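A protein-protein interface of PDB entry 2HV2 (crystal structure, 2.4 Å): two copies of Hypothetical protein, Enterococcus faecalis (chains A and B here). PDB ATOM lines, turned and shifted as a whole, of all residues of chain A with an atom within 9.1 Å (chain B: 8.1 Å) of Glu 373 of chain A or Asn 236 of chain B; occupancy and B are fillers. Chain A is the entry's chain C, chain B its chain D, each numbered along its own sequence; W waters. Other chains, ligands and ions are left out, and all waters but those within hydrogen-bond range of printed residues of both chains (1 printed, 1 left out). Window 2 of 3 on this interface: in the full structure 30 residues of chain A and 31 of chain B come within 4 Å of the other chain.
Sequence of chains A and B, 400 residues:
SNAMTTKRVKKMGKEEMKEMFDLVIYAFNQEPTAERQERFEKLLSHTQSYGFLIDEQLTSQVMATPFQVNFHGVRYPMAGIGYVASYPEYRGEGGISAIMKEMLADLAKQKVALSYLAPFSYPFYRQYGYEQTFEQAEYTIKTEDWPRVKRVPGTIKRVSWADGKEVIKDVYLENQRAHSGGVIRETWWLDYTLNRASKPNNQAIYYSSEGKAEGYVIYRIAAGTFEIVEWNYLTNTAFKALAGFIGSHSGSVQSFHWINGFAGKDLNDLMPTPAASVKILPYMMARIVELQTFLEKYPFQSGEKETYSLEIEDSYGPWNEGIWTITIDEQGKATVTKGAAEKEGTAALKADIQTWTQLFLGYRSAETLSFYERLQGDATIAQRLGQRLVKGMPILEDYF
OH of Tyr 372 of chain A sits at hydrogen-bond distance from OH of Tyr 233 of chain B (3.0 Å).
OE1 of Glu 373 of chain A lies within hydrogen-bond range of ND2 of Asn 236 of chain B (3.0 Å).
The guanidinium group (NH2) of Arg 374 of chain A is in hydrogen-bond range of the backbone carbonyl oxygen (O) of Leu 270 of chain B, at 3.2 Å.
No position is printed for both chains.
Of the 10 pairs that touch across the chains among the printed residues, none has its exchanged pair printed and touching as well.
Hydrophobic or aromatic side chains of chain A within 4 Å of the printed part of chain B: Phe 371 and Tyr 372.
Of the 16 printed residues of chain B, 6 touch a printed residue of chain A.
Hydrophobic or aromatic side chains of chain B that line the printed part of chain A: Tyr 233, Phe 239 and Leu 270.
Water W1 bridges N of Asn 236 of chain B (2.8 Å) and O of Phe 371 of chain A (2.9 Å).
Among the printed residues, pairs that only touch across the chains: Phe 371 of chain A with Asn 236 of chain B (3.2 Å), Phe 371 of chain A with Leu 234 of chain B (3.3 Å), Tyr 372 of chain A with Asn 236 of chain B (3.5 Å), Tyr 372 of chain A with Leu 270 of chain B (3.7 Å), Phe 371 of chain A with Thr 235 of chain B (3.8 Å), Phe 371 of chain A with Tyr 233 of chain B (3.9 Å) and Tyr 372 of chain A with Phe 239 of chain B (3.997 Å).
The backbone carbonyl oxygen (O) of Leu 369 of chain A sits at hydrogen-bond distance from the backbone NH (N) of Arg 374 of chain A, at 2.9 Å.
N of Leu 234 of chain B sits at hydrogen-bond distance from O of Glu 214 of chain B (2.8 Å).
The side-chain carboxylate (OE1) of Glu 214 of chain B is in hydrogen-bond range of the side-chain hydroxyl (OG1) of Thr 235 of chain B (2.9 Å).
The side-chain hydroxyl of Thr 235 of chain B is in hydrogen-bond range of the backbone NH of Ala 238 of chain B (3.2 Å).
NZ of Lys 240 of chain B sits close to ND2 of Asn 236 of chain B (3.1 Å).
Glu 367 of chain A touches none of the printed residues of chain B.
Printed residues of chain B within 4 Å of Phe 371 of chain A: Tyr 233, Leu 234, Thr 235 and Asn 236.
Of the printed residues of chain B, Tyr 372 of chain A touches Tyr 233 (3.0 Å), Asn 236 (3.5 Å), Phe 239 (3.997 Å) and Leu 270 (3.7 Å).
Glu 373 of chain A touches one residue of chain B.
Of the printed residues of chain B, Arg 374 of chain A touches Leu 270 (3.2 Å).
Gly 377 of chain A touches none of the printed residues of chain B.
Of the printed residues of chain A, Thr 235 of chain B touches Phe 371 (3.8 Å).
Of chain A, only Phe 371, Tyr 372 and Glu 373 come within 4 Å of Asn 236 of chain B.
No residue of chain A comes within 4 Å of Thr 237 of chain B.
Of the printed residues of chain A, Phe 239 of chain B touches Tyr 372 (3.997 Å).
Of the printed residues of chain A, Leu 270 of chain B touches Tyr 372 and Arg 374.
The nearest residue of chain A that does not touch Asn 236 of chain B is Ser 370 of chain A (6.1 Å).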
ATOM      1  N   LYS A 350       3.077 -25.624 -13.620  1.00  0.00           N
ATOM      2  CA  LYS A 350       3.494 -24.524 -12.741  1.00  0.00           C
ATOM      3  C   LYS A 350       3.034 -23.172 -13.297  1.00  0.00           C
ATOM      4  O   LYS A 350       3.208 -22.886 -14.458  1.00  0.00           O
ATOM      5  CB  LYS A 350       5.023 -24.557 -12.574  1.00  0.00           C
ATOM      6  CG  LYS A 350       5.589 -23.498 -11.640  1.00  0.00           C
ATOM      7  CD  LYS A 350       7.109 -23.470 -11.683  1.00  0.00           C
ATOM      8  CE  LYS A 350       7.678 -22.323 -10.857  1.00  0.00           C
ATOM      9  NZ  LYS A 350       9.137 -22.109 -11.087  1.00  0.00           N
ATOM     10  N   ALA A 351       2.458 -22.287 -12.498  1.00  0.00           N
ATOM     11  CA  ALA A 351       2.027 -20.946 -12.937  1.00  0.00           C
ATOM     12  C   ALA A 351       1.908 -20.019 -11.758  1.00  0.00           C
ATOM     13  O   ALA A 351       1.865 -20.445 -10.612  1.00  0.00           O
ATOM     14  CB  ALA A 351       0.676 -20.998 -13.661  1.00  0.00           C
ATOM     15  N   ASP A 352       1.814 -18.718 -12.000  1.00  0.00           N
ATOM     16  CA  ASP A 352       1.524 -17.746 -10.962  1.00  0.00           C
ATOM     17  C   ASP A 352       0.014 -17.602 -10.810  1.00  0.00           C
ATOM     18  O   ASP A 352      -0.736 -17.974 -11.700  1.00  0.00           O
ATOM     19  CB  ASP A 352       2.218 -16.419 -11.255  1.00  0.00           C
ATOM     20  CG  ASP A 352       1.834 -15.817 -12.587  1.00  0.00           C
ATOM     21  OD1 ASP A 352       2.556 -14.868 -13.004  1.00  0.00           O
ATOM     22  OD2 ASP A 352       0.863 -16.194 -13.299  1.00  0.00           O
ATOM     23  N   THR A 355      -2.104 -16.400 -13.967  1.00  0.00           N
ATOM     24  CA  THR A 355      -2.345 -17.343 -15.025  1.00  0.00           C
ATOM     25  C   THR A 355      -3.325 -18.401 -14.622  1.00  0.00           C
ATOM     26  O   THR A 355      -4.082 -18.874 -15.469  1.00  0.00           O
ATOM     27  CB  THR A 355      -1.019 -18.024 -15.396  1.00  0.00           C
ATOM     28  OG1 THR A 355      -0.122 -17.029 -15.892  1.00  0.00           O
ATOM     29  CG2 THR A 355      -1.222 -19.140 -16.425  1.00  0.00           C
ATOM     30  N   ALA A 366      -5.785 -23.577 -22.095  1.00  0.00           N
ATOM     31  CA  ALA A 366      -4.563 -24.232 -21.671  1.00  0.00           C
ATOM     32  C   ALA A 366      -3.549 -24.122 -22.787  1.00  0.00           C
ATOM     33  O   ALA A 366      -2.389 -23.789 -22.542  1.00  0.00           O
ATOM     34  CB  ALA A 366      -4.817 -25.708 -21.336  1.00  0.00           C
ATOM     35  N   GLU A 367      -3.948 -24.340 -24.039  1.00  0.00           N
ATOM     36  CA  GLU A 367      -3.052 -24.349 -25.196  1.00  0.00           C
ATOM     37  C   GLU A 367      -2.375 -22.993 -25.340  1.00  0.00           C
ATOM     38  O   GLU A 367      -1.155 -22.904 -25.442  1.00  0.00           O
ATOM     39  CB  GLU A 367      -3.828 -24.680 -26.476  1.00  0.00           C
ATOM     40  CG  GLU A 367      -4.686 -25.959 -26.392  1.00  0.00           C
ATOM     41  CD  GLU A 367      -6.103 -25.729 -25.807  1.00  0.00           C
ATOM     42  OE1 GLU A 367      -7.066 -25.520 -26.616  1.00  0.00           O
ATOM     43  OE2 GLU A 367      -6.258 -25.761 -24.544  1.00  0.00           O
ATOM     44  N   THR A 368      -3.119 -21.904 -25.331  1.00  0.00           N
ATOM     45  CA  THR A 368      -2.592 -20.576 -25.473  1.00  0.00           C
ATOM     46  C   THR A 368      -1.620 -20.231 -24.353  1.00  0.00           C
ATOM     47  O   THR A 368      -0.545 -19.696 -24.602  1.00  0.00           O
ATOM     48  CB  THR A 368      -3.761 -19.588 -25.424  1.00  0.00           C
ATOM     49  OG1 THR A 368      -4.343 -19.476 -26.725  1.00  0.00           O
ATOM     50  CG2 THR A 368      -3.299 -18.233 -24.938  1.00  0.00           C
ATOM     51  N   LEU A 369      -1.950 -20.505 -23.096  1.00  0.00           N
ATOM     52  CA  LEU A 369      -1.118 -20.121 -21.957  1.00  0.00           C
ATOM     53  C   LEU A 369       0.089 -21.022 -21.886  1.00  0.00           C
ATOM     54  O   LEU A 369       1.144 -20.621 -21.399  1.00  0.00           O
ATOM     55  CB  LEU A 369      -1.944 -20.201 -20.674  1.00  0.00           C
ATOM     56  CG  LEU A 369      -3.035 -19.137 -20.538  1.00  0.00           C
ATOM     57  CD1 LEU A 369      -4.052 -19.548 -19.476  1.00  0.00           C
ATOM     58  CD2 LEU A 369      -2.400 -17.786 -20.190  1.00  0.00           C
ATOM     59  N   SER A 370      -0.001 -22.255 -22.377  1.00  0.00           N
ATOM     60  CA  SER A 370       1.147 -23.128 -22.530  1.00  0.00           C
ATOM     61  C   SER A 370       2.089 -22.604 -23.624  1.00  0.00           C
ATOM     62  O   SER A 370       3.306 -22.571 -23.436  1.00  0.00           O
ATOM     63  CB  SER A 370       0.674 -24.540 -22.902  1.00  0.00           C
ATOM     64  OG  SER A 370       1.745 -25.458 -22.892  1.00  0.00           O
ATOM     65  N   PHE A 371       1.583 -22.197 -24.790  1.00  0.00           N
ATOM     66  CA  PHE A 371       2.397 -21.724 -25.903  1.00  0.00           C
ATOM     67  C   PHE A 371       3.180 -20.490 -25.520  1.00  0.00           C
ATOM     68  O   PHE A 371       4.386 -20.424 -25.733  1.00  0.00           O
ATOM     69  CB  PHE A 371       1.501 -21.390 -27.075  1.00  0.00           C
ATOM     70  CG  PHE A 371       2.233 -20.894 -28.280  1.00  0.00           C
ATOM     71  CD1 PHE A 371       2.467 -19.563 -28.451  1.00  0.00           C
ATOM     72  CD2 PHE A 371       2.655 -21.762 -29.237  1.00  0.00           C
ATOM     73  CE1 PHE A 371       3.123 -19.106 -29.543  1.00  0.00           C
ATOM     74  CE2 PHE A 371       3.303 -21.310 -30.350  1.00  0.00           C
ATOM     75  CZ  PHE A 371       3.543 -19.979 -30.499  1.00  0.00           C
ATOM     76  N   TYR A 372       2.542 -19.486 -24.926  1.00  0.00           N
ATOM     77  CA  TYR A 372       3.202 -18.268 -24.478  1.00  0.00           C
ATOM     78  C   TYR A 372       3.944 -18.490 -23.159  1.00  0.00           C
ATOM     79  O   TYR A 372       4.364 -17.511 -22.528  1.00  0.00           O
ATOM     80  CB  TYR A 372       2.184 -17.127 -24.370  1.00  0.00           C
ATOM     81  CG  TYR A 372       1.616 -16.699 -25.719  1.00  0.00           C
ATOM     82  CD1 TYR A 372       2.409 -16.065 -26.659  1.00  0.00           C
ATOM     83  CD2 TYR A 372       0.291 -16.951 -26.053  1.00  0.00           C
ATOM     84  CE1 TYR A 372       1.903 -15.681 -27.892  1.00  0.00           C
ATOM     85  CE2 TYR A 372      -0.236 -16.576 -27.279  1.00  0.00           C
ATOM     86  CZ  TYR A 372       0.578 -15.945 -28.204  1.00  0.00           C
ATOM     87  OH  TYR A 372       0.067 -15.580 -29.442  1.00  0.00           O
ATOM     88  N   GLU A 373       4.133 -19.749 -22.720  1.00  0.00           N
ATOM     89  CA  GLU A 373       4.978 -20.173 -21.591  1.00  0.00           C
ATOM     90  C   GLU A 373       4.576 -19.554 -20.241  1.00  0.00           C
ATOM     91  O   GLU A 373       5.419 -19.362 -19.365  1.00  0.00           O
ATOM     92  CB  GLU A 373       6.476 -19.932 -21.910  1.00  0.00           C
ATOM     93  CG  GLU A 373       7.026 -20.859 -23.017  1.00  0.00           C
ATOM     94  CD  GLU A 373       8.446 -20.519 -23.471  1.00  0.00           C
ATOM     95  OE1 GLU A 373       8.950 -19.437 -23.075  1.00  0.00           O
ATOM     96  OE2 GLU A 373       9.061 -21.308 -24.253  1.00  0.00           O
ATOM     97  N   ARG A 374       3.304 -19.250 -20.010  1.00  0.00           N
ATOM     98  CA  ARG A 374       2.801 -18.838 -18.702  1.00  0.00           C
ATOM     99  C   ARG A 374       2.359 -20.037 -17.871  1.00  0.00           C
ATOM    100  O   ARG A 374       2.533 -20.065 -16.649  1.00  0.00           O
ATOM    101  CB  ARG A 374       1.633 -17.895 -18.888  1.00  0.00           C
ATOM    102  CG  ARG A 374       1.973 -16.789 -19.847  1.00  0.00           C
ATOM    103  CD  ARG A 374       1.214 -15.508 -19.635  1.00  0.00           C
ATOM    104  NE  ARG A 374       1.801 -14.432 -20.436  1.00  0.00           N
ATOM    105  CZ  ARG A 374       1.256 -13.228 -20.588  1.00  0.00           C
ATOM    106  NH1 ARG A 374       0.100 -12.941 -19.986  1.00  0.00           N
ATOM    107  NH2 ARG A 374       1.873 -12.307 -21.341  1.00  0.00           N
ATOM    108  N   LEU A 375       1.750 -21.039 -18.491  1.00  0.00           N
ATOM    109  CA  LEU A 375       1.490 -22.326 -17.896  1.00  0.00           C
ATOM    110  C   LEU A 375       2.677 -23.211 -18.279  1.00  0.00           C
ATOM    111  O   LEU A 375       2.852 -23.582 -19.436  1.00  0.00           O
ATOM    112  CB  LEU A 375       0.147 -22.856 -18.411  1.00  0.00           C
ATOM    113  CG  LEU A 375      -0.395 -24.171 -17.838  1.00  0.00           C
ATOM    114  CD1 LEU A 375      -0.611 -24.071 -16.354  1.00  0.00           C
ATOM    115  CD2 LEU A 375      -1.691 -24.551 -18.542  1.00  0.00           C
ATOM    116  N   GLN A 376       3.558 -23.541 -17.350  1.00  0.00           N
ATOM    117  CA  GLN A 376       4.748 -24.319 -17.630  1.00  0.00           C
ATOM    118  C   GLN A 376       4.544 -25.780 -17.259  1.00  0.00           C
ATOM    119  O   GLN A 376       3.945 -26.096 -16.227  1.00  0.00           O
ATOM    120  CB  GLN A 376       5.939 -23.803 -16.824  1.00  0.00           C
ATOM    121  CG  GLN A 376       6.396 -22.404 -17.176  1.00  0.00           C
ATOM    122  CD  GLN A 376       6.934 -21.672 -15.951  1.00  0.00           C
ATOM    123  OE1 GLN A 376       7.814 -22.182 -15.233  1.00  0.00           O
ATOM    124  NE2 GLN A 376       6.383 -20.494 -15.693  1.00  0.00           N
ATOM    125  N   GLY A 377       5.111 -26.696 -18.037  1.00  0.00           N
ATOM    126  CA  GLY A 377       5.034 -28.120 -17.836  1.00  0.00           C
ATOM    127  C   GLY A 377       4.712 -28.744 -19.176  1.00  0.00           C
ATOM    128  O   GLY A 377       4.429 -28.031 -20.161  1.00  0.00           O
ATOM    129  N   VAL B 149      10.572  -5.510 -24.339  1.00  0.00           N
ATOM    130  CA  VAL B 149      10.667  -6.962 -24.330  1.00  0.00           C
ATOM    131  C   VAL B 149      12.098  -7.294 -24.018  1.00  0.00           C
ATOM    132  O   VAL B 149      12.975  -6.846 -24.738  1.00  0.00           O
ATOM    133  CB  VAL B 149      10.325  -7.564 -25.714  1.00  0.00           C
ATOM    134  CG1 VAL B 149      10.195  -9.078 -25.640  1.00  0.00           C
ATOM    135  CG2 VAL B 149       9.055  -6.945 -26.276  1.00  0.00           C
ATOM    136  N   VAL B 152      16.363 -12.280 -25.991  1.00  0.00           N
ATOM    137  CA  VAL B 152      15.974 -13.688 -25.894  1.00  0.00           C
ATOM    138  C   VAL B 152      16.957 -14.510 -26.754  1.00  0.00           C
ATOM    139  O   VAL B 152      17.603 -13.962 -27.632  1.00  0.00           O
ATOM    140  CB  VAL B 152      14.478 -13.836 -26.292  1.00  0.00           C
ATOM    141  CG1 VAL B 152      14.283 -14.535 -27.627  1.00  0.00           C
ATOM    142  CG2 VAL B 152      13.699 -14.562 -25.202  1.00  0.00           C
ATOM    143  N   TYR B 206      13.289 -15.106 -37.666  1.00  0.00           N
ATOM    144  CA  TYR B 206      13.839 -15.548 -36.411  1.00  0.00           C
ATOM    145  C   TYR B 206      14.384 -16.966 -36.556  1.00  0.00           C
ATOM    146  O   TYR B 206      13.688 -17.860 -37.080  1.00  0.00           O
ATOM    147  CB  TYR B 206      12.793 -15.504 -35.285  1.00  0.00           C
ATOM    148  CG  TYR B 206      13.313 -16.102 -33.992  1.00  0.00           C
ATOM    149  CD1 TYR B 206      14.220 -15.400 -33.195  1.00  0.00           C
ATOM    150  CD2 TYR B 206      12.967 -17.392 -33.614  1.00  0.00           C
ATOM    151  CE1 TYR B 206      14.734 -15.949 -32.037  1.00  0.00           C
ATOM    152  CE2 TYR B 206      13.484 -17.961 -32.456  1.00  0.00           C
ATOM    153  CZ  TYR B 206      14.353 -17.225 -31.667  1.00  0.00           C
ATOM    154  OH  TYR B 206      14.843 -17.759 -30.515  1.00  0.00           O
ATOM    155  N   GLU B 214      11.956 -20.191 -36.701  1.00  0.00           N
ATOM    156  CA  GLU B 214      10.739 -20.347 -35.907  1.00  0.00           C
ATOM    157  C   GLU B 214       9.795 -19.176 -36.104  1.00  0.00           C
ATOM    158  O   GLU B 214       8.718 -19.166 -35.517  1.00  0.00           O
ATOM    159  CB  GLU B 214      11.074 -20.520 -34.410  1.00  0.00           C
ATOM    160  CG  GLU B 214      12.118 -21.593 -34.157  1.00  0.00           C
ATOM    161  CD  GLU B 214      12.206 -22.078 -32.707  1.00  0.00           C
ATOM    162  OE1 GLU B 214      12.138 -21.251 -31.746  1.00  0.00           O
ATOM    163  OE2 GLU B 214      12.388 -23.310 -32.523  1.00  0.00           O
ATOM    164  N   TYR B 233       4.727 -16.759 -35.874  1.00  0.00           N
ATOM    165  CA  TYR B 233       5.702 -17.331 -34.986  1.00  0.00           C
ATOM    166  C   TYR B 233       5.258 -18.734 -34.543  1.00  0.00           C
ATOM    167  O   TYR B 233       4.071 -18.981 -34.336  1.00  0.00           O
ATOM    168  CB  TYR B 233       5.980 -16.386 -33.808  1.00  0.00           C
ATOM    169  CG  TYR B 233       4.757 -15.767 -33.226  1.00  0.00           C
ATOM    170  CD1 TYR B 233       4.012 -16.428 -32.241  1.00  0.00           C
ATOM    171  CD2 TYR B 233       4.320 -14.526 -33.660  1.00  0.00           C
ATOM    172  CE1 TYR B 233       2.859 -15.849 -31.712  1.00  0.00           C
ATOM    173  CE2 TYR B 233       3.167 -13.945 -33.141  1.00  0.00           C
ATOM    174  CZ  TYR B 233       2.451 -14.605 -32.167  1.00  0.00           C
ATOM    175  OH  TYR B 233       1.328 -14.030 -31.658  1.00  0.00           O
ATOM    176  N   LEU B 234       6.197 -19.681 -34.426  1.00  0.00           N
ATOM    177  CA  LEU B 234       5.961 -21.069 -34.055  1.00  0.00           C
ATOM    178  C   LEU B 234       6.309 -21.314 -32.585  1.00  0.00           C
ATOM    179  O   LEU B 234       5.935 -22.341 -32.037  1.00  0.00           O
ATOM    180  CB  LEU B 234       6.822 -21.986 -34.935  1.00  0.00           C
ATOM    181  CG  LEU B 234       6.637 -21.826 -36.456  1.00  0.00           C
ATOM    182  CD1 LEU B 234       7.744 -22.522 -37.206  1.00  0.00           C
ATOM    183  CD2 LEU B 234       5.256 -22.344 -36.886  1.00  0.00           C
ATOM    184  N   THR B 235       7.025 -20.425 -31.895  1.00  0.00           N
ATOM    185  CA  THR B 235       7.360 -20.611 -30.501  1.00  0.00           C
ATOM    186  C   THR B 235       7.242 -19.301 -29.752  1.00  0.00           C
ATOM    187  O   THR B 235       7.270 -18.230 -30.350  1.00  0.00           O
ATOM    188  CB  THR B 235       8.801 -21.126 -30.347  1.00  0.00           C
ATOM    189  OG1 THR B 235       9.725 -20.083 -30.702  1.00  0.00           O
ATOM    190  CG2 THR B 235       9.043 -22.371 -31.200  1.00  0.00           C
ATOM    191  N   ASN B 236       7.126 -19.319 -28.435  1.00  0.00           N
ATOM    192  CA  ASN B 236       7.130 -18.111 -27.636  1.00  0.00           C
ATOM    193  C   ASN B 236       8.422 -17.326 -27.739  1.00  0.00           C
ATOM    194  O   ASN B 236       8.383 -16.109 -27.671  1.00  0.00           O
ATOM    195  CB  ASN B 236       6.912 -18.437 -26.160  1.00  0.00           C
ATOM    196  CG  ASN B 236       6.792 -17.194 -25.312  1.00  0.00           C
ATOM    197  OD1 ASN B 236       5.950 -16.340 -25.586  1.00  0.00           O
ATOM    198  ND2 ASN B 236       7.638 -17.075 -24.291  1.00  0.00           N
ATOM    199  N   THR B 237       9.602 -17.924 -27.869  1.00  0.00           N
ATOM    200  CA  THR B 237      10.823 -17.108 -27.910  1.00  0.00           C
ATOM    201  C   THR B 237      10.971 -16.442 -29.326  1.00  0.00           C
ATOM    202  O   THR B 237      11.469 -15.305 -29.403  1.00  0.00           O
ATOM    203  CB  THR B 237      12.101 -17.840 -27.303  1.00  0.00           C
ATOM    204  OG1 THR B 237      13.236 -17.765 -28.182  1.00  0.00           O
ATOM    205  CG2 THR B 237      11.829 -19.284 -26.926  1.00  0.00           C
ATOM    206  N   ALA B 238      10.457 -17.017 -30.426  1.00  0.00           N
ATOM    207  CA  ALA B 238      10.304 -16.312 -31.704  1.00  0.00           C
ATOM    208  C   ALA B 238       9.367 -15.089 -31.579  1.00  0.00           C
ATOM    209  O   ALA B 238       9.662 -14.001 -32.088  1.00  0.00           O
ATOM    210  CB  ALA B 238       9.774 -17.249 -32.774  1.00  0.00           C
ATOM    211  N   PHE B 239       8.214 -15.227 -30.935  1.00  0.00           N
ATOM    212  CA  PHE B 239       7.308 -14.133 -30.612  1.00  0.00           C
ATOM    213  C   PHE B 239       7.991 -12.989 -29.871  1.00  0.00           C
ATOM    214  O   PHE B 239       7.890 -11.847 -30.286  1.00  0.00           O
ATOM    215  CB  PHE B 239       6.184 -14.683 -29.746  1.00  0.00           C
ATOM    216  CG  PHE B 239       5.234 -13.641 -29.239  1.00  0.00           C
ATOM    217  CD1 PHE B 239       4.422 -12.974 -30.102  1.00  0.00           C
ATOM    218  CD2 PHE B 239       5.155 -13.357 -27.897  1.00  0.00           C
ATOM    219  CE1 PHE B 239       3.544 -12.038 -29.658  1.00  0.00           C
ATOM    220  CE2 PHE B 239       4.271 -12.422 -27.438  1.00  0.00           C
ATOM    221  CZ  PHE B 239       3.473 -11.753 -28.321  1.00  0.00           C
ATOM    222  N   LYS B 240       8.695 -13.243 -28.773  1.00  0.00           N
ATOM    223  CA  LYS B 240       9.400 -12.224 -27.987  1.00  0.00           C
ATOM    224  C   LYS B 240      10.571 -11.603 -28.750  1.00  0.00           C
ATOM    225  O   LYS B 240      10.787 -10.393 -28.673  1.00  0.00           O
ATOM    226  CB  LYS B 240       9.925 -12.843 -26.684  1.00  0.00           C
ATOM    227  CG  LYS B 240       8.873 -13.010 -25.601  1.00  0.00           C
ATOM    228  CD  LYS B 240       9.070 -14.282 -24.790  1.00  0.00           C
ATOM    229  CE  LYS B 240       9.611 -14.061 -23.382  1.00  0.00           C
ATOM    230  NZ  LYS B 240       9.161 -15.122 -22.430  1.00  0.00           N
ATOM    231  N   ALA B 241      11.356 -12.382 -29.493  1.00  0.00           N
ATOM    232  CA  ALA B 241      12.481 -11.880 -30.298  1.00  0.00           C
ATOM    233  C   ALA B 241      11.949 -10.894 -31.309  1.00  0.00           C
ATOM    234  O   ALA B 241      12.464  -9.767 -31.433  1.00  0.00           O
ATOM    235  CB  ALA B 241      13.194 -13.031 -31.020  1.00  0.00           C
ATOM    236  N   LEU B 242      10.920 -11.255 -32.065  1.00  0.00           N
ATOM    237  CA  LEU B 242      10.424 -10.421 -33.139  1.00  0.00           C
ATOM    238  C   LEU B 242       9.665  -9.228 -32.555  1.00  0.00           C
ATOM    239  O   LEU B 242       9.698  -8.147 -33.104  1.00  0.00           O
ATOM    240  CB  LEU B 242       9.534 -11.242 -34.097  1.00  0.00           C
ATOM    241  CG  LEU B 242      10.264 -12.290 -34.982  1.00  0.00           C
ATOM    242  CD1 LEU B 242       9.312 -13.354 -35.503  1.00  0.00           C
ATOM    243  CD2 LEU B 242      10.995 -11.649 -36.161  1.00  0.00           C
ATOM    244  N   ALA B 243       8.970  -9.367 -31.431  1.00  0.00           N
ATOM    245  CA  ALA B 243       8.279  -8.269 -30.760  1.00  0.00           C
ATOM    246  C   ALA B 243       9.323  -7.225 -30.399  1.00  0.00           C
ATOM    247  O   ALA B 243       9.094  -6.042 -30.585  1.00  0.00           O
ATOM    248  CB  ALA B 243       7.532  -8.771 -29.493  1.00  0.00           C
ATOM    249  N   LEU B 270      -1.608  -9.873 -23.717  1.00  0.00           N
ATOM    250  CA  LEU B 270      -0.213 -10.302 -23.587  1.00  0.00           C
ATOM    251  C   LEU B 270       0.685  -9.144 -23.148  1.00  0.00           C
ATOM    252  O   LEU B 270       1.768  -9.381 -22.651  1.00  0.00           O
ATOM    253  CB  LEU B 270       0.314 -10.875 -24.916  1.00  0.00           C
ATOM    254  CG  LEU B 270      -0.494 -12.035 -25.541  1.00  0.00           C
ATOM    255  CD1 LEU B 270       0.225 -12.589 -26.756  1.00  0.00           C
ATOM    256  CD2 LEU B 270      -0.773 -13.117 -24.531  1.00  0.00           C
HETATM  257  O   HOH W   1       6.416 -21.717 -27.289  1.00  0.00           O
